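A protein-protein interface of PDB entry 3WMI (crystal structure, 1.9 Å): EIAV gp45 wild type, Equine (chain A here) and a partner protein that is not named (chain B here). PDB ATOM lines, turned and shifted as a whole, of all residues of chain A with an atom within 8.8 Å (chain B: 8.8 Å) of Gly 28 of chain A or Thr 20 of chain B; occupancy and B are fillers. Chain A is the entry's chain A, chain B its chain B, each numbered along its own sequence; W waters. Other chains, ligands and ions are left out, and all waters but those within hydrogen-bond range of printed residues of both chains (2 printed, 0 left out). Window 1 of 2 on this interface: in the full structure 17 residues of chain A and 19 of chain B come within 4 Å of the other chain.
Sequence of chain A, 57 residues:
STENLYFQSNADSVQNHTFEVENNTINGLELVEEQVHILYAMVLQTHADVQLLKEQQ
The side-chain amide nitrogen (ND2) of Asn 27 of chain B lies within hydrogen-bond range of the side-chain amide oxygen (OD1) of Asn 24 of chain A (2.9 Å). NE2 of Gln 35 of chain A is in hydrogen-bond range of OD1 of Asn 14 of chain B.
The side-chain hydroxyl (OG1) of Thr 25 of chain A is in hydrogen-bond range of the backbone carbonyl oxygen (O) of Val 21 of chain A. OG1 of Thr 19 of chain B is in hydrogen-bond range of O of Asp 16 of chain B (2.9 Å). The side-chain hydroxyl (OG1) of Thr 20 of chain B sits at hydrogen-bond distance from the backbone carbonyl oxygen (O) of Asp 16 of chain B, 2.8 Å away. ND2 of Asn 27 of chain B sits at hydrogen-bond distance from O of Thr 23 of chain B, at 3.4 Å. The backbone carbonyl oxygen of Glu 20 of chain A lies close to the side-chain amide oxygen of Asn 24 of chain A, 3.0 Å away. The backbone carbonyl oxygen (O) of Thr 19 of chain B is in hydrogen-bond range of the side-chain hydroxyl (OG1) of Thr 23 of chain B, 3.0 Å away.
Asn 27 of chain B touches Glu 20 of chain A. CG2 of Val 21 of chain A touches O of Ala 24 of chain B (3.8 Å). Asn 24 of chain A touches Thr 20 of chain B (O to CG2, 3.2 Å). OD1 of Asn 24 of chain A touches CG2 of Thr 23 of chain B, 3.5 Å away. Asn 24 of chain A touches Ala 24 of chain B. CG2 of Thr 20 of chain B touches N of Gly 28 of chain A, 3.9 Å away. CD2 of Leu 31 of chain A touches CD1 of Leu 13 of chain B (3.8 Å). Ile 17 of chain B touches Leu 31 of chain A (CG1 to CB, 3.5 Å). Leu 31 of chain A touches Thr 20 of chain B (CD1 to OG1, 3.6 Å). Leu 13 of chain B touches Glu 34 of chain A.
Of the printed residues of chain B, Val 21 of chain A touches Ala 24 (3.8 Å) and Asn 27 (3.7 Å). Asn 27 of chain A touches none of the printed residues of chain B. Gly 28 of chain A touches one residue of chain B. Printed residues of chain B within 4 Å of Gln 35 of chain A: Leu 13 (3.6 Å), Asn 14 (2.9 Å) and Ile 17 (3.0 Å). Printed residues of chain A within 4 Å of Ile 17 of chain B: Leu 31 (3.5 Å), Val 32 (3.8 Å) and Gln 35 (3.0 Å). Thr 19 of chain B touches none of the printed residues of chain A. Thr 20 of chain B touches three residues of chain A. Asn 26 of chain B touches none of the printed residues of chain A. The nearest printed residue of chain A that does not touch Asn 27 of chain B is Glu 22 of chain A (7.0 Å).
Printed residues of chain B that touch a printed residue of chain A: Leu 13, Asn 14, Asp 16, Ile 17, Thr 20, Thr 23, Ala 24 and Asn 27. Hydrophobic or aromatic side chains of chain B that line the printed part of chain A: Leu 13, Ile 17 and Ala 24. Printed residues of chain A that touch a printed residue of chain B: Glu 20, Val 21, Asn 24, Gly 28, Leu 31, Val 32, Glu 34 and Gln 35. Among the printed residues, 17 pairs touch across the chains. Among the printed residues, no Asp or Glu carboxylate lies within 4 Å of a Lys or Arg side-chain nitrogen of the other chain.
Water W2 lies within hydrogen-bond range of the side-chain carboxylate of Glu 20 of chain A (2.6 Å) and the side-chain amide oxygen of Asn 27 of chain B (2.8 Å). Water W1 bridges the side-chain amide nitrogen of Asn 24 of chain A (3.1 Å) and the side-chain amide nitrogen of Asn 27 of chain B (3.3 Å).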
ATOM      1  N   GLU A  20      18.717  30.103  -7.029  1.00  0.00           N
ATOM      2  CA  GLU A  20      19.649  30.642  -6.036  1.00  0.00           C
ATOM      3  C   GLU A  20      20.433  29.541  -5.313  1.00  0.00           C
ATOM      4  O   GLU A  20      21.641  29.667  -5.131  1.00  0.00           O
ATOM      5  CB  GLU A  20      18.951  31.584  -5.039  1.00  0.00           C
ATOM      6  CG  GLU A  20      18.387  32.844  -5.697  1.00  0.00           C
ATOM      7  CD  GLU A  20      17.840  33.872  -4.713  1.00  0.00           C
ATOM      8  OE1 GLU A  20      16.875  33.570  -3.977  1.00  0.00           O
ATOM      9  OE2 GLU A  20      18.373  35.004  -4.693  1.00  0.00           O
ATOM     10  N   VAL A  21      19.755  28.470  -4.906  1.00  0.00           N
ATOM     11  CA  VAL A  21      20.443  27.325  -4.280  1.00  0.00           C
ATOM     12  C   VAL A  21      21.512  26.774  -5.220  1.00  0.00           C
ATOM     13  O   VAL A  21      22.637  26.458  -4.807  1.00  0.00           O
ATOM     14  CB  VAL A  21      19.477  26.180  -3.931  1.00  0.00           C
ATOM     15  CG1 VAL A  21      20.257  24.938  -3.499  1.00  0.00           C
ATOM     16  CG2 VAL A  21      18.512  26.595  -2.833  1.00  0.00           C
ATOM     17  N   GLU A  22      21.160  26.664  -6.496  1.00  0.00           N
ATOM     18  CA  GLU A  22      22.100  26.176  -7.492  1.00  0.00           C
ATOM     19  C   GLU A  22      23.319  27.086  -7.649  1.00  0.00           C
ATOM     20  O   GLU A  22      24.462  26.609  -7.665  1.00  0.00           O
ATOM     21  CB  GLU A  22      21.377  25.958  -8.822  1.00  0.00           C
ATOM     22  CG  GLU A  22      20.462  24.750  -8.749  1.00  0.00           C
ATOM     23  CD  GLU A  22      19.695  24.504 -10.026  1.00  0.00           C
ATOM     24  OE1 GLU A  22      19.633  25.398 -10.886  1.00  0.00           O
ATOM     25  OE2 GLU A  22      19.149  23.393 -10.155  1.00  0.00           O
ATOM     26  N   ASN A  23      23.071  28.389  -7.753  1.00  0.00           N
ATOM     27  CA  ASN A  23      24.149  29.382  -7.769  1.00  0.00           C
ATOM     28  C   ASN A  23      25.031  29.341  -6.508  1.00  0.00           C
ATOM     29  O   ASN A  23      26.265  29.389  -6.613  1.00  0.00           O
ATOM     30  CB  ASN A  23      23.591  30.794  -7.989  1.00  0.00           C
ATOM     31  CG  ASN A  23      24.681  31.862  -7.994  1.00  0.00           C
ATOM     32  OD1 ASN A  23      25.571  31.843  -8.838  1.00  0.00           O
ATOM     33  ND2 ASN A  23      24.611  32.788  -7.053  1.00  0.00           N
ATOM     34  N   ASN A  24      24.410  29.242  -5.331  1.00  0.00           N
ATOM     35  CA  ASN A  24      25.164  29.137  -4.074  1.00  0.00           C
ATOM     36  C   ASN A  24      26.071  27.911  -4.086  1.00  0.00           C
ATOM     37  O   ASN A  24      27.214  27.963  -3.644  1.00  0.00           O
ATOM     38  CB  ASN A  24      24.252  29.030  -2.838  1.00  0.00           C
ATOM     39  CG  ASN A  24      23.316  30.226  -2.655  1.00  0.00           C
ATOM     40  OD1 ASN A  24      22.179  30.060  -2.207  1.00  0.00           O
ATOM     41  ND2 ASN A  24      23.788  31.425  -2.978  1.00  0.00           N
ATOM     42  N   THR A  25      25.543  26.800  -4.577  1.00  0.00           N
ATOM     43  CA  THR A  25      26.254  25.532  -4.523  1.00  0.00           C
ATOM     44  C   THR A  25      27.420  25.502  -5.521  1.00  0.00           C
ATOM     45  O   THR A  25      28.506  24.999  -5.213  1.00  0.00           O
ATOM     46  CB  THR A  25      25.298  24.360  -4.768  1.00  0.00           C
ATOM     47  OG1 THR A  25      24.219  24.430  -3.826  1.00  0.00           O
ATOM     48  CG2 THR A  25      26.024  23.065  -4.552  1.00  0.00           C
ATOM     49  N   ILE A  26      27.192  26.048  -6.710  1.00  0.00           N
ATOM     50  CA  ILE A  26      28.268  26.194  -7.696  1.00  0.00           C
ATOM     51  C   ILE A  26      29.333  27.125  -7.136  1.00  0.00           C
ATOM     52  O   ILE A  26      30.528  26.844  -7.235  1.00  0.00           O
ATOM     53  CB  ILE A  26      27.749  26.718  -9.048  1.00  0.00           C
ATOM     54  CG1 ILE A  26      26.769  25.717  -9.666  1.00  0.00           C
ATOM     55  CG2 ILE A  26      28.902  26.965 -10.015  1.00  0.00           C
ATOM     56  CD1 ILE A  26      25.897  26.351 -10.768  1.00  0.00           C
ATOM     57  N   ASN A  27      28.898  28.226  -6.526  1.00  0.00           N
ATOM     58  CA  ASN A  27      29.836  29.164  -5.915  1.00  0.00           C
ATOM     59  C   ASN A  27      30.666  28.524  -4.791  1.00  0.00           C
ATOM     60  O   ASN A  27      31.873  28.768  -4.683  1.00  0.00           O
ATOM     61  CB  ASN A  27      29.110  30.411  -5.407  1.00  0.00           C
ATOM     62  CG  ASN A  27      28.768  31.382  -6.522  1.00  0.00           C
ATOM     63  OD1 ASN A  27      29.272  31.260  -7.632  1.00  0.00           O
ATOM     64  ND2 ASN A  27      27.920  32.361  -6.224  1.00  0.00           N
ATOM     65  N   GLY A  28      30.014  27.717  -3.960  1.00  0.00           N
ATOM     66  CA  GLY A  28      30.691  27.015  -2.875  1.00  0.00           C
ATOM     67  C   GLY A  28      31.732  26.042  -3.402  1.00  0.00           C
ATOM     68  O   GLY A  28      32.852  25.966  -2.881  1.00  0.00           O
ATOM     69  N   LEU A  29      31.369  25.306  -4.446  1.00  0.00           N
ATOM     70  CA  LEU A  29      32.310  24.410  -5.101  1.00  0.00           C
ATOM     71  C   LEU A  29      33.516  25.181  -5.588  1.00  0.00           C
ATOM     72  O   LEU A  29      34.652  24.743  -5.403  1.00  0.00           O
ATOM     73  CB  LEU A  29      31.662  23.714  -6.292  1.00  0.00           C
ATOM     74  CG  LEU A  29      31.125  22.319  -6.033  1.00  0.00           C
ATOM     75  CD1 LEU A  29      30.428  21.801  -7.291  1.00  0.00           C
ATOM     76  CD2 LEU A  29      32.276  21.410  -5.626  1.00  0.00           C
ATOM     77  N   GLU A  30      33.283  26.333  -6.214  1.00  0.00           N
ATOM     78  CA  GLU A  30      34.403  27.129  -6.714  1.00  0.00           C
ATOM     79  C   GLU A  30      35.311  27.612  -5.590  1.00  0.00           C
ATOM     80  O   GLU A  30      36.536  27.622  -5.736  1.00  0.00           O
ATOM     81  CB  GLU A  30      33.934  28.322  -7.539  1.00  0.00           C
ATOM     82  CG  GLU A  30      35.107  29.107  -8.112  1.00  0.00           C
ATOM     83  CD  GLU A  30      34.882  29.533  -9.550  1.00  0.00           C
ATOM     84  OE1 GLU A  30      33.775  30.020  -9.853  1.00  0.00           O
ATOM     85  OE2 GLU A  30      35.808  29.379 -10.373  1.00  0.00           O
ATOM     86  N   LEU A  31      34.711  28.015  -4.477  1.00  0.00           N
ATOM     87  CA  LEU A  31      35.491  28.461  -3.325  1.00  0.00           C
ATOM     88  C   LEU A  31      36.323  27.316  -2.747  1.00  0.00           C
ATOM     89  O   LEU A  31      37.474  27.514  -2.401  1.00  0.00           O
ATOM     90  CB  LEU A  31      34.590  29.052  -2.243  1.00  0.00           C
ATOM     91  CG  LEU A  31      33.886  30.361  -2.608  1.00  0.00           C
ATOM     92  CD1 LEU A  31      32.807  30.644  -1.590  1.00  0.00           C
ATOM     93  CD2 LEU A  31      34.891  31.488  -2.657  1.00  0.00           C
ATOM     94  N   VAL A  32      35.726  26.135  -2.619  1.00  0.00           N
ATOM     95  CA  VAL A  32      36.453  24.968  -2.127  1.00  0.00           C
ATOM     96  C   VAL A  32      37.622  24.668  -3.057  1.00  0.00           C
ATOM     97  O   VAL A  32      38.735  24.384  -2.600  1.00  0.00           O
ATOM     98  CB  VAL A  32      35.536  23.734  -1.991  1.00  0.00           C
ATOM     99  CG1 VAL A  32      36.343  22.477  -1.795  1.00  0.00           C
ATOM    100  CG2 VAL A  32      34.523  23.934  -0.848  1.00  0.00           C
ATOM    101  N   GLU A  33      37.382  24.769  -4.358  1.00  0.00           N
ATOM    102  CA  GLU A  33      38.442  24.561  -5.347  1.00  0.00           C
ATOM    103  C   GLU A  33      39.591  25.564  -5.201  1.00  0.00           C
ATOM    104  O   GLU A  33      40.750  25.216  -5.426  1.00  0.00           O
ATOM    105  CB  GLU A  33      37.885  24.586  -6.775  1.00  0.00           C
ATOM    106  CG  GLU A  33      38.934  24.346  -7.877  1.00  0.00           C
ATOM    107  CD  GLU A  33      39.524  22.931  -7.857  1.00  0.00           C
ATOM    108  OE1 GLU A  33      39.141  22.116  -6.988  1.00  0.00           O
ATOM    109  OE2 GLU A  33      40.369  22.631  -8.725  1.00  0.00           O
ATOM    110  N   GLU A  34      39.280  26.798  -4.817  1.00  0.00           N
ATOM    111  CA  GLU A  34      40.338  27.782  -4.575  1.00  0.00           C
ATOM    112  C   GLU A  34      41.167  27.379  -3.357  1.00  0.00           C
ATOM    113  O   GLU A  34      42.388  27.555  -3.345  1.00  0.00           O
ATOM    114  CB  GLU A  34      39.765  29.192  -4.397  1.00  0.00           C
ATOM    115  CG  GLU A  34      39.090  29.743  -5.652  1.00  0.00           C
ATOM    116  CD  GLU A  34      38.569  31.158  -5.472  1.00  0.00           C
ATOM    117  OE1 GLU A  34      39.053  31.863  -4.557  1.00  0.00           O
ATOM    118  OE2 GLU A  34      37.667  31.568  -6.244  1.00  0.00           O
ATOM    119  N   GLN A  35      40.498  26.845  -2.340  1.00  0.00           N
ATOM    120  CA  GLN A  35      41.200  26.293  -1.186  1.00  0.00           C
ATOM    121  C   GLN A  35      42.106  25.129  -1.595  1.00  0.00           C
ATOM    122  O   GLN A  35      43.212  25.012  -1.092  1.00  0.00           O
ATOM    123  CB  GLN A  35      40.220  25.826  -0.120  1.00  0.00           C
ATOM    124  CG  GLN A  35      39.438  26.939   0.536  1.00  0.00           C
ATOM    125  CD  GLN A  35      38.549  26.395   1.607  1.00  0.00           C
ATOM    126  OE1 GLN A  35      37.860  25.417   1.382  1.00  0.00           O
ATOM    127  NE2 GLN A  35      38.583  26.990   2.785  1.00  0.00           N
ATOM    128  N   ASN B  12      40.220  33.544   4.857  1.00  0.00           N
ATOM    129  CA  ASN B  12      39.150  34.303   4.219  1.00  0.00           C
ATOM    130  C   ASN B  12      38.190  33.398   3.452  1.00  0.00           C
ATOM    131  O   ASN B  12      36.971  33.592   3.485  1.00  0.00           O
ATOM    132  CB  ASN B  12      39.735  35.366   3.301  1.00  0.00           C
ATOM    133  CG  ASN B  12      40.428  36.462   4.068  1.00  0.00           C
ATOM    134  OD1 ASN B  12      40.212  36.619   5.271  1.00  0.00           O
ATOM    135  ND2 ASN B  12      41.264  37.231   3.382  1.00  0.00           N
ATOM    136  N   LEU B  13      38.746  32.406   2.763  1.00  0.00           N
ATOM    137  CA  LEU B  13      37.940  31.399   2.079  1.00  0.00           C
ATOM    138  C   LEU B  13      37.077  30.591   3.066  1.00  0.00           C
ATOM    139  O   LEU B  13      35.927  30.269   2.769  1.00  0.00           O
ATOM    140  CB  LEU B  13      38.853  30.460   1.289  1.00  0.00           C
ATOM    141  CG  LEU B  13      38.981  30.579  -0.238  1.00  0.00           C
ATOM    142  CD1 LEU B  13      38.198  31.736  -0.825  1.00  0.00           C
ATOM    143  CD2 LEU B  13      40.436  30.595  -0.698  1.00  0.00           C
ATOM    144  N   ASN B  14      37.643  30.236   4.219  1.00  0.00           N
ATOM    145  CA  ASN B  14      36.870  29.580   5.279  1.00  0.00           C
ATOM    146  C   ASN B  14      35.595  30.357   5.560  1.00  0.00           C
ATOM    147  O   ASN B  14      34.491  29.794   5.586  1.00  0.00           O
ATOM    148  CB  ASN B  14      37.674  29.461   6.582  1.00  0.00           C
ATOM    149  CG  ASN B  14      38.705  28.351   6.547  1.00  0.00           C
ATOM    150  OD1 ASN B  14      38.735  27.530   5.629  1.00  0.00           O
ATOM    151  ND2 ASN B  14      39.553  28.307   7.573  1.00  0.00           N
ATOM    152  N   HIS B  15      35.745  31.660   5.761  1.00  0.00           N
ATOM    153  CA  HIS B  15      34.595  32.495   6.081  1.00  0.00           C
ATOM    154  C   HIS B  15      33.599  32.549   4.920  1.00  0.00           C
ATOM    155  O   HIS B  15      32.393  32.402   5.130  1.00  0.00           O
ATOM    156  CB  HIS B  15      35.046  33.902   6.465  1.00  0.00           C
ATOM    157  CG  HIS B  15      33.916  34.854   6.689  1.00  0.00           C
ATOM    158  ND1 HIS B  15      33.062  34.757   7.769  1.00  0.00           N
ATOM    159  CD2 HIS B  15      33.493  35.920   5.969  1.00  0.00           C
ATOM    160  CE1 HIS B  15      32.167  35.724   7.705  1.00  0.00           C
ATOM    161  NE2 HIS B  15      32.405  36.446   6.624  1.00  0.00           N
ATOM    162  N   ASP B  16      34.112  32.751   3.707  1.00  0.00           N
ATOM    163  CA  ASP B  16      33.280  32.803   2.506  1.00  0.00           C
ATOM    164  C   ASP B  16      32.446  31.533   2.344  1.00  0.00           C
ATOM    165  O   ASP B  16      31.267  31.588   1.992  1.00  0.00           O
ATOM    166  CB  ASP B  16      34.139  32.959   1.247  1.00  0.00           C
ATOM    167  CG  ASP B  16      34.828  34.312   1.146  1.00  0.00           C
ATOM    168  OD1 ASP B  16      34.389  35.264   1.815  1.00  0.00           O
ATOM    169  OD2 ASP B  16      35.808  34.414   0.373  1.00  0.00           O
ATOM    170  N   ILE B  17      33.064  30.381   2.569  1.00  0.00           N
ATOM    171  CA  ILE B  17      32.365  29.108   2.378  1.00  0.00           C
ATOM    172  C   ILE B  17      31.301  28.894   3.456  1.00  0.00           C
ATOM    173  O   ILE B  17      30.197  28.420   3.174  1.00  0.00           O
ATOM    174  CB  ILE B  17      33.358  27.936   2.345  1.00  0.00           C
ATOM    175  CG1 ILE B  17      34.168  28.014   1.060  1.00  0.00           C
ATOM    176  CG2 ILE B  17      32.632  26.614   2.415  1.00  0.00           C
ATOM    177  CD1 ILE B  17      35.369  27.127   1.029  1.00  0.00           C
ATOM    178  N   LEU B  18      31.632  29.260   4.691  1.00  0.00           N
ATOM    179  CA  LEU B  18      30.665  29.200   5.787  1.00  0.00           C
ATOM    180  C   LEU B  18      29.415  30.001   5.461  1.00  0.00           C
ATOM    181  O   LEU B  18      28.297  29.530   5.651  1.00  0.00           O
ATOM    182  CB  LEU B  18      31.285  29.741   7.080  1.00  0.00           C
ATOM    183  CG  LEU B  18      31.917  28.727   8.028  1.00  0.00           C
ATOM    184  CD1 LEU B  18      32.694  29.434   9.140  1.00  0.00           C
ATOM    185  CD2 LEU B  18      30.832  27.857   8.611  1.00  0.00           C
ATOM    186  N   THR B  19      29.604  31.220   4.970  1.00  0.00           N
ATOM    187  CA  THR B  19      28.466  32.085   4.665  1.00  0.00           C
ATOM    188  C   THR B  19      27.700  31.574   3.453  1.00  0.00           C
ATOM    189  O   THR B  19      26.467  31.664   3.399  1.00  0.00           O
ATOM    190  CB  THR B  19      28.898  33.554   4.460  1.00  0.00           C
ATOM    191  OG1 THR B  19      29.746  33.658   3.310  1.00  0.00           O
ATOM    192  CG2 THR B  19      29.666  34.042   5.673  1.00  0.00           C
ATOM    193  N   THR B  20      28.428  31.021   2.488  1.00  0.00           N
ATOM    194  CA  THR B  20      27.814  30.487   1.280  1.00  0.00           C
ATOM    195  C   THR B  20      26.933  29.276   1.595  1.00  0.00           C
ATOM    196  O   THR B  20      25.813  29.171   1.090  1.00  0.00           O
ATOM    197  CB  THR B  20      28.874  30.126   0.211  1.00  0.00           C
ATOM    198  OG1 THR B  20      29.525  31.316  -0.244  1.00  0.00           O
ATOM    199  CG2 THR B  20      28.224  29.449  -0.989  1.00  0.00           C
ATOM    200  N   LEU B  21      27.429  28.367   2.429  1.00  0.00           N
ATOM    201  CA  LEU B  21      26.644  27.199   2.827  1.00  0.00           C
ATOM    202  C   LEU B  21      25.399  27.614   3.596  1.00  0.00           C
ATOM    203  O   LEU B  21      24.327  27.074   3.365  1.00  0.00           O
ATOM    204  CB  LEU B  21      27.473  26.219   3.665  1.00  0.00           C
ATOM    205  CG  LEU B  21      28.648  25.553   2.940  1.00  0.00           C
ATOM    206  CD1 LEU B  21      29.478  24.725   3.901  1.00  0.00           C
ATOM    207  CD2 LEU B  21      28.155  24.697   1.800  1.00  0.00           C
ATOM    208  N   HIS B  22      25.540  28.575   4.506  1.00  0.00           N
ATOM    209  CA  HIS B  22      24.381  29.073   5.251  1.00  0.00           C
ATOM    210  C   HIS B  22      23.318  29.649   4.302  1.00  0.00           C
ATOM    211  O   HIS B  22      22.125  29.387   4.447  1.00  0.00           O
ATOM    212  CB  HIS B  22      24.808  30.126   6.280  1.00  0.00           C
ATOM    213  CG  HIS B  22      23.697  30.579   7.178  1.00  0.00           C
ATOM    214  ND1 HIS B  22      22.839  31.608   6.842  1.00  0.00           N
ATOM    215  CD2 HIS B  22      23.297  30.141   8.394  1.00  0.00           C
ATOM    216  CE1 HIS B  22      21.963  31.782   7.814  1.00  0.00           C
ATOM    217  NE2 HIS B  22      22.219  30.905   8.769  1.00  0.00           N
ATOM    218  N   THR B  23      23.768  30.424   3.327  1.00  0.00           N
ATOM    219  CA  THR B  23      22.881  31.030   2.354  1.00  0.00           C
ATOM    220  C   THR B  23      22.152  29.966   1.540  1.00  0.00           C
ATOM    221  O   THR B  23      20.941  30.049   1.365  1.00  0.00           O
ATOM    222  CB  THR B  23      23.665  31.960   1.429  1.00  0.00           C
ATOM    223  OG1 THR B  23      24.140  33.075   2.192  1.00  0.00           O
ATOM    224  CG2 THR B  23      22.797  32.454   0.282  1.00  0.00           C
ATOM    225  N   ALA B  24      22.896  28.971   1.063  1.00  0.00           N
ATOM    226  CA  ALA B  24      22.326  27.847   0.320  1.00  0.00           C
ATOM    227  C   ALA B  24      21.247  27.150   1.128  1.00  0.00           C
ATOM    228  O   ALA B  24      20.157  26.893   0.622  1.00  0.00           O
ATOM    229  CB  ALA B  24      23.419  26.851  -0.067  1.00  0.00           C
ATOM    230  N   ARG B  25      21.541  26.847   2.387  1.00  0.00           N
ATOM    231  CA  ARG B  25      20.573  26.133   3.220  1.00  0.00           C
ATOM    232  C   ARG B  25      19.334  26.992   3.472  1.00  0.00           C
ATOM    233  O   ARG B  25      18.208  26.487   3.500  1.00  0.00           O
ATOM    234  CB  ARG B  25      21.205  25.658   4.545  1.00  0.00           C
ATOM    235  CG  ARG B  25      22.207  24.495   4.371  1.00  0.00           C
ATOM    236  CD  ARG B  25      22.624  23.861   5.703  1.00  0.00           C
ATOM    237  NE  ARG B  25      23.406  22.639   5.502  1.00  0.00           N
ATOM    238  CZ  ARG B  25      24.683  22.498   5.849  1.00  0.00           C
ATOM    239  NH1 ARG B  25      25.330  23.504   6.430  1.00  0.00           N
ATOM    240  NH2 ARG B  25      25.319  21.349   5.624  1.00  0.00           N
ATOM    241  N   ASN B  26      19.548  28.290   3.647  1.00  0.00           N
ATOM    242  CA  ASN B  26      18.447  29.214   3.851  1.00  0.00           C
ATOM    243  C   ASN B  26      17.540  29.334   2.626  1.00  0.00           C
ATOM    244  O   ASN B  26      16.312  29.354   2.753  1.00  0.00           O
ATOM    245  CB  ASN B  26      18.964  30.590   4.258  1.00  0.00           C
ATOM    246  CG  ASN B  26      17.854  31.514   4.669  1.00  0.00           C
ATOM    247  OD1 ASN B  26      17.565  32.499   3.994  1.00  0.00           O
ATOM    248  ND2 ASN B  26      17.195  31.178   5.771  1.00  0.00           N
ATOM    249  N   ASN B  27      18.140  29.426   1.443  1.00  0.00           N
ATOM    250  CA  ASN B  27      17.364  29.439   0.211  1.00  0.00           C
ATOM    251  C   ASN B  27      16.597  28.138  -0.006  1.00  0.00           C
ATOM    252  O   ASN B  27      15.446  28.156  -0.432  1.00  0.00           O
ATOM    253  CB  ASN B  27      18.255  29.780  -0.988  1.00  0.00           C
ATOM    254  CG  ASN B  27      18.632  31.248  -1.017  1.00  0.00           C
ATOM    255  OD1 ASN B  27      17.831  32.111  -0.654  1.00  0.00           O
ATOM    256  ND2 ASN B  27      19.853  31.539  -1.433  1.00  0.00           N
HETATM  257  O   HOH W   1      21.826  33.811  -2.717  1.00  0.00           O
HETATM  258  O   HOH W   2      17.133  34.627  -1.571  1.00  0.00           O
